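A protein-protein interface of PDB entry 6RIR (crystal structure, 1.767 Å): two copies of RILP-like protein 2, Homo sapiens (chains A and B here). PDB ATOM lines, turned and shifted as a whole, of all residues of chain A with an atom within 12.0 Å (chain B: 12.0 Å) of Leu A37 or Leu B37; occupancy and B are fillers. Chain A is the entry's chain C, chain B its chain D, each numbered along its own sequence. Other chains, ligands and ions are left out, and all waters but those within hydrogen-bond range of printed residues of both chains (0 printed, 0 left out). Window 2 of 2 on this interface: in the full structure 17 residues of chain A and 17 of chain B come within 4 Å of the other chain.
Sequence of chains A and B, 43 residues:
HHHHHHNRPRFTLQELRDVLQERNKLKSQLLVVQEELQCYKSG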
ATOM      1  N   SER A  28       8.292 -10.742  25.988  1.00  0.00           N
ATOM      2  CA  SER A  28       8.848 -11.464  24.844  1.00  0.00           C
ATOM      3  C   SER A  28      10.368 -11.400  24.840  1.00  0.00           C
ATOM      4  O   SER A  28      11.040 -12.429  24.700  1.00  0.00           O
ATOM      5  CB  SER A  28       8.288 -10.908  23.535  1.00  0.00           C
ATOM      6  OG  SER A  28       6.901 -11.156  23.429  1.00  0.00           O
ATOM      7  N   GLN A  29      10.930 -10.194  24.980  1.00  0.00           N
ATOM      8  CA  GLN A  29      12.383 -10.055  25.057  1.00  0.00           C
ATOM      9  C   GLN A  29      12.965 -10.942  26.153  1.00  0.00           C
ATOM     10  O   GLN A  29      14.003 -11.588  25.955  1.00  0.00           O
ATOM     11  CB  GLN A  29      12.769  -8.590  25.299  1.00  0.00           C
ATOM     12  CG  GLN A  29      12.304  -7.602  24.223  1.00  0.00           C
ATOM     13  CD  GLN A  29      12.552  -6.145  24.616  1.00  0.00           C
ATOM     14  OE1 GLN A  29      13.673  -5.760  24.948  1.00  0.00           O
ATOM     15  NE2 GLN A  29      11.500  -5.338  24.595  1.00  0.00           N
ATOM     16  N   LEU A  30      12.303 -11.000  27.312  1.00  0.00           N
ATOM     17  CA  LEU A  30      12.814 -11.806  28.417  1.00  0.00           C
ATOM     18  C   LEU A  30      12.779 -13.296  28.085  1.00  0.00           C
ATOM     19  O   LEU A  30      13.757 -14.017  28.318  1.00  0.00           O
ATOM     20  CB  LEU A  30      12.015 -11.520  29.687  1.00  0.00           C
ATOM     21  CG  LEU A  30      12.327 -12.482  30.836  1.00  0.00           C
ATOM     22  CD1 LEU A  30      13.789 -12.338  31.262  1.00  0.00           C
ATOM     23  CD2 LEU A  30      11.376 -12.263  32.010  1.00  0.00           C
ATOM     24  N   LEU A  31      11.650 -13.781  27.559  1.00  0.00           N
ATOM     25  CA  LEU A  31      11.552 -15.194  27.196  1.00  0.00           C
ATOM     26  C   LEU A  31      12.623 -15.580  26.181  1.00  0.00           C
ATOM     27  O   LEU A  31      13.196 -16.673  26.256  1.00  0.00           O
ATOM     28  CB  LEU A  31      10.154 -15.504  26.652  1.00  0.00           C
ATOM     29  CG  LEU A  31       8.980 -15.379  27.630  1.00  0.00           C
ATOM     30  CD1 LEU A  31       7.659 -15.156  26.890  1.00  0.00           C
ATOM     31  CD2 LEU A  31       8.884 -16.589  28.544  1.00  0.00           C
ATOM     32  N   VAL A  32      12.921 -14.684  25.238  1.00  0.00           N
ATOM     33  CA  VAL A  32      13.941 -14.956  24.225  1.00  0.00           C
ATOM     34  C   VAL A  32      15.306 -15.159  24.876  1.00  0.00           C
ATOM     35  O   VAL A  32      15.963 -16.186  24.675  1.00  0.00           O
ATOM     36  CB  VAL A  32      13.984 -13.823  23.185  1.00  0.00           C
ATOM     37  CG1 VAL A  32      15.322 -13.813  22.461  1.00  0.00           C
ATOM     38  CG2 VAL A  32      12.847 -13.972  22.191  1.00  0.00           C
ATOM     39  N   VAL A  33      15.764 -14.174  25.654  1.00  0.00           N
ATOM     40  CA  VAL A  33      17.112 -14.269  26.204  1.00  0.00           C
ATOM     41  C   VAL A  33      17.197 -15.371  27.252  1.00  0.00           C
ATOM     42  O   VAL A  33      18.275 -15.934  27.481  1.00  0.00           O
ATOM     43  CB  VAL A  33      17.573 -12.913  26.769  1.00  0.00           C
ATOM     44  CG1 VAL A  33      17.388 -11.823  25.731  1.00  0.00           C
ATOM     45  CG2 VAL A  33      16.803 -12.574  28.033  1.00  0.00           C
ATOM     46  N   GLN A  34      16.073 -15.714  27.886  1.00  0.00           N
ATOM     47  CA  GLN A  34      16.078 -16.789  28.874  1.00  0.00           C
ATOM     48  C   GLN A  34      16.391 -18.136  28.231  1.00  0.00           C
ATOM     49  O   GLN A  34      17.065 -18.975  28.839  1.00  0.00           O
ATOM     50  CB  GLN A  34      14.734 -16.848  29.600  1.00  0.00           C
ATOM     51  CG  GLN A  34      14.711 -16.097  30.920  1.00  0.00           C
ATOM     52  CD  GLN A  34      13.325 -16.004  31.512  1.00  0.00           C
ATOM     53  OE1 GLN A  34      12.334 -16.344  30.863  1.00  0.00           O
ATOM     54  NE2 GLN A  34      13.243 -15.538  32.751  1.00  0.00           N
ATOM     55  N   GLU A  35      15.910 -18.367  27.010  1.00  0.00           N
ATOM     56  CA  GLU A  35      16.152 -19.641  26.346  1.00  0.00           C
ATOM     57  C   GLU A  35      17.463 -19.664  25.574  1.00  0.00           C
ATOM     58  O   GLU A  35      17.816 -20.710  25.018  1.00  0.00           O
ATOM     59  CB  GLU A  35      14.989 -19.999  25.412  1.00  0.00           C
ATOM     60  CG  GLU A  35      14.645 -18.955  24.371  1.00  0.00           C
ATOM     61  CD  GLU A  35      13.348 -19.266  23.652  1.00  0.00           C
ATOM     62  OE1 GLU A  35      12.565 -20.089  24.173  1.00  0.00           O
ATOM     63  OE2 GLU A  35      13.109 -18.690  22.568  1.00  0.00           O
ATOM     64  N   GLU A  36      18.204 -18.552  25.538  1.00  0.00           N
ATOM     65  CA  GLU A  36      19.572 -18.587  25.024  1.00  0.00           C
ATOM     66  C   GLU A  36      20.526 -19.316  25.969  1.00  0.00           C
ATOM     67  O   GLU A  36      21.750 -19.267  25.787  1.00  0.00           O
ATOM     68  CB  GLU A  36      20.077 -17.168  24.761  1.00  0.00           C
ATOM     69  CG  GLU A  36      19.141 -16.326  23.909  1.00  0.00           C
ATOM     70  CD  GLU A  36      19.851 -15.173  23.223  1.00  0.00           C
ATOM     71  OE1 GLU A  36      19.157 -14.267  22.711  1.00  0.00           O
ATOM     72  OE2 GLU A  36      21.100 -15.175  23.193  1.00  0.00           O
ATOM     73  N   LEU A  37      19.958 -19.979  26.972  1.00  0.00           N
ATOM     74  CA  LEU A  37      20.710 -20.739  27.960  1.00  0.00           C
ATOM     75  C   LEU A  37      20.224 -22.189  28.009  1.00  0.00           C
ATOM     76  O   LEU A  37      20.867 -23.094  27.470  1.00  0.00           O
ATOM     77  CB  LEU A  37      20.579 -20.085  29.337  1.00  0.00           C
ATOM     78  CG  LEU A  37      20.523 -18.555  29.299  1.00  0.00           C
ATOM     79  CD1 LEU A  37      20.072 -17.961  30.628  1.00  0.00           C
ATOM     80  CD2 LEU A  37      21.878 -18.015  28.902  1.00  0.00           C
ATOM     81  N   SER B  28      13.754  -5.317  35.010  1.00  0.00           N
ATOM     82  CA  SER B  28      14.839  -5.724  35.893  1.00  0.00           C
ATOM     83  C   SER B  28      15.285  -7.146  35.590  1.00  0.00           C
ATOM     84  O   SER B  28      16.487  -7.425  35.498  1.00  0.00           O
ATOM     85  CB  SER B  28      14.395  -5.605  37.352  1.00  0.00           C
ATOM     86  OG  SER B  28      14.355  -4.242  37.741  1.00  0.00           O
ATOM     87  N   GLN B  29      14.324  -8.066  35.451  1.00  0.00           N
ATOM     88  CA  GLN B  29      14.659  -9.448  35.114  1.00  0.00           C
ATOM     89  C   GLN B  29      15.376  -9.538  33.771  1.00  0.00           C
ATOM     90  O   GLN B  29      16.328 -10.312  33.623  1.00  0.00           O
ATOM     91  CB  GLN B  29      13.392 -10.306  35.103  1.00  0.00           C
ATOM     92  CG  GLN B  29      12.779 -10.501  36.477  1.00  0.00           C
ATOM     93  CD  GLN B  29      11.435 -11.198  36.420  1.00  0.00           C
ATOM     94  OE1 GLN B  29      10.649 -10.986  35.496  1.00  0.00           O
ATOM     95  NE2 GLN B  29      11.162 -12.031  37.412  1.00  0.00           N
ATOM     96  N   LEU B  30      14.935  -8.755  32.780  1.00  0.00           N
ATOM     97  CA  LEU B  30      15.580  -8.776  31.468  1.00  0.00           C
ATOM     98  C   LEU B  30      17.027  -8.312  31.556  1.00  0.00           C
ATOM     99  O   LEU B  30      17.931  -8.953  31.004  1.00  0.00           O
ATOM    100  CB  LEU B  30      14.810  -7.902  30.475  1.00  0.00           C
ATOM    101  CG  LEU B  30      15.475  -7.681  29.110  1.00  0.00           C
ATOM    102  CD1 LEU B  30      15.585  -8.994  28.339  1.00  0.00           C
ATOM    103  CD2 LEU B  30      14.726  -6.633  28.285  1.00  0.00           C
ATOM    104  N   LEU B  31      17.262  -7.181  32.225  1.00  0.00           N
ATOM    105  CA  LEU B  31      18.621  -6.665  32.340  1.00  0.00           C
ATOM    106  C   LEU B  31      19.536  -7.667  33.027  1.00  0.00           C
ATOM    107  O   LEU B  31      20.719  -7.764  32.678  1.00  0.00           O
ATOM    108  CB  LEU B  31      18.616  -5.335  33.098  1.00  0.00           C
ATOM    109  CG  LEU B  31      17.966  -4.143  32.393  1.00  0.00           C
ATOM    110  CD1 LEU B  31      17.863  -2.936  33.328  1.00  0.00           C
ATOM    111  CD2 LEU B  31      18.725  -3.772  31.121  1.00  0.00           C
ATOM    112  N   VAL B  32      19.006  -8.435  33.982  1.00  0.00           N
ATOM    113  CA  VAL B  32      19.834  -9.386  34.721  1.00  0.00           C
ATOM    114  C   VAL B  32      20.286 -10.523  33.809  1.00  0.00           C
ATOM    115  O   VAL B  32      21.480 -10.839  33.728  1.00  0.00           O
ATOM    116  CB  VAL B  32      19.077  -9.917  35.955  1.00  0.00           C
ATOM    117  CG1 VAL B  32      19.614 -11.277  36.376  1.00  0.00           C
ATOM    118  CG2 VAL B  32      19.182  -8.927  37.103  1.00  0.00           C
ATOM    119  N   VAL B  33      19.339 -11.157  33.113  1.00  0.00           N
ATOM    120  CA  VAL B  33      19.712 -12.255  32.227  1.00  0.00           C
ATOM    121  C   VAL B  33      20.584 -11.752  31.079  1.00  0.00           C
ATOM    122  O   VAL B  33      21.475 -12.472  30.606  1.00  0.00           O
ATOM    123  CB  VAL B  33      18.450 -12.982  31.727  1.00  0.00           C
ATOM    124  CG1 VAL B  33      18.817 -14.057  30.707  1.00  0.00           C
ATOM    125  CG2 VAL B  33      17.703 -13.600  32.903  1.00  0.00           C
ATOM    126  N   GLN B  34      20.375 -10.509  30.633  1.00  0.00           N
ATOM    127  CA  GLN B  34      21.229  -9.947  29.588  1.00  0.00           C
ATOM    128  C   GLN B  34      22.682  -9.890  30.040  1.00  0.00           C
ATOM    129  O   GLN B  34      23.574 -10.422  29.368  1.00  0.00           O
ATOM    130  CB  GLN B  34      20.738  -8.555  29.187  1.00  0.00           C
ATOM    131  CG  GLN B  34      19.549  -8.584  28.241  1.00  0.00           C
ATOM    132  CD  GLN B  34      19.096  -7.205  27.821  1.00  0.00           C
ATOM    133  OE1 GLN B  34      19.286  -6.226  28.543  1.00  0.00           O
ATOM    134  NE2 GLN B  34      18.472  -7.122  26.658  1.00  0.00           N
ATOM    135  N   GLU B  35      22.940  -9.256  31.187  1.00  0.00           N
ATOM    136  CA  GLU B  35      24.309  -9.118  31.670  1.00  0.00           C
ATOM    137  C   GLU B  35      24.920 -10.456  32.070  1.00  0.00           C
ATOM    138  O   GLU B  35      26.150 -10.580  32.084  1.00  0.00           O
ATOM    139  CB  GLU B  35      24.361  -8.143  32.846  1.00  0.00           C
ATOM    140  CG  GLU B  35      23.792  -8.687  34.147  1.00  0.00           C
ATOM    141  CD  GLU B  35      23.814  -7.661  35.267  1.00  0.00           C
ATOM    142  OE1 GLU B  35      24.562  -6.668  35.150  1.00  0.00           O
ATOM    143  OE2 GLU B  35      23.080  -7.848  36.264  1.00  0.00           O
ATOM    144  N   GLU B  36      24.100 -11.460  32.377  1.00  0.00           N
ATOM    145  CA  GLU B  36      24.640 -12.766  32.732  1.00  0.00           C
ATOM    146  C   GLU B  36      25.246 -13.503  31.551  1.00  0.00           C
ATOM    147  O   GLU B  36      25.649 -14.661  31.711  1.00  0.00           O
ATOM    148  CB  GLU B  36      23.559 -13.635  33.367  1.00  0.00           C
ATOM    149  CG  GLU B  36      23.326 -13.338  34.830  1.00  0.00           C
ATOM    150  CD  GLU B  36      22.790 -14.539  35.576  1.00  0.00           C
ATOM    151  OE1 GLU B  36      23.482 -15.580  35.604  1.00  0.00           O
ATOM    152  OE2 GLU B  36      21.676 -14.443  36.132  1.00  0.00           O
ATOM    153  N   LEU B  37      25.312 -12.885  30.378  1.00  0.00           N
ATOM    154  CA  LEU B  37      25.986 -13.492  29.234  1.00  0.00           C
ATOM    155  C   LEU B  37      27.370 -12.869  29.062  1.00  0.00           C
ATOM    156  O   LEU B  37      27.699 -12.223  28.065  1.00  0.00           O
ATOM    157  CB  LEU B  37      25.128 -13.363  27.978  1.00  0.00           C
ATOM    158  CG  LEU B  37      23.637 -13.710  28.131  1.00  0.00           C
ATOM    159  CD1 LEU B  37      23.003 -14.003  26.780  1.00  0.00           C
ATOM    160  CD2 LEU B  37      23.402 -14.885  29.073  1.00  0.00           C
ATOM    161  N   GLN B  38      28.168 -13.067  30.107  1.00  0.00           N
ATOM    162  CA  GLN B  38      29.570 -12.689  30.141  1.00  0.00           C
ATOM    163  C   GLN B  38      30.409 -13.957  30.122  1.00  0.00           C
ATOM    164  O   GLN B  38      29.882 -15.055  30.321  1.00  0.00           O
ATOM    165  CB  GLN B  38      29.875 -11.857  31.387  1.00  0.00           C
ATOM    166  CG  GLN B  38      29.015 -12.233  32.592  1.00  0.00           C
ATOM    167  CD  GLN B  38      29.244 -11.332  33.795  1.00  0.00           C
ATOM    168  OE1 GLN B  38      29.441 -10.125  33.653  1.00  0.00           O
ATOM    169  NE2 GLN B  38      29.208 -11.917  34.989  1.00  0.00           N
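Of chain B, only Leu B37 (3.5 Å) comes within 4 Å of Leu A37. Of chain A, only Leu A37 (3.5 Å) comes within 4 Å of Leu B37. Of chain B, only Leu B30 and Val B33 come within 4 Å of Val A33. No residue of chain B comes within 4 Å of Glu A36. Val B33 touches just one residue of chain A: Val A33 (3.7 Å). No residue of chain A comes within 4 Å of Glu B36. Gln B38 touches none of the printed residues of chain A. Of the printed residues of chain B, Leu A30 touches Gln B29 (3.8 Å) and Leu B30 (3.9 Å). Printed residues of chain A within 4 Å of Leu B30: Gln A29 (3.6 Å), Leu A30 (3.9 Å) and Val A33 (3.8 Å). Printed residues of chain A within 4 Å of Gln B29: Leu A30 (3.8 Å). Printed residues of chain B within 4 Å of Gln A29: Leu B30. Ser A28 touches none of the printed residues of chain B. Glu B35 touches none of the printed residues of chain A. The nearest residue of chain B that does not touch Leu A37 is Val B33 (4.1 Å). The nearest residue of chain A that does not touch Leu B37 is Glu A36 (4.2 Å). The nearest printed residue of chain A that does not touch Leu B30 is Leu A31 (6.2 Å).
Among the printed residues, pairs that only touch across the chains: Gln A29 with Leu B30, Leu A30 with Gln B29, Leu A30 with Leu B30, Val A33 with Leu B30, Val A33 with Val B33 and Leu A37 with Leu B37.
Of the 10 printed residues of chain A, 4 touch a printed residue of chain B.
Leu B30 touches its own counterpart, Leu A30. Val A33 touches Leu B30, but with the chains exchanged Leu A30 does not touch Val B33 (4.4 Å). Val A33 touches its own counterpart, Val B33. Leu A37 touches its own counterpart, Leu B37. Of the 6 pairs that touch across the chains among the printed residues, 5 have their exchanged pair printed and touching as well.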
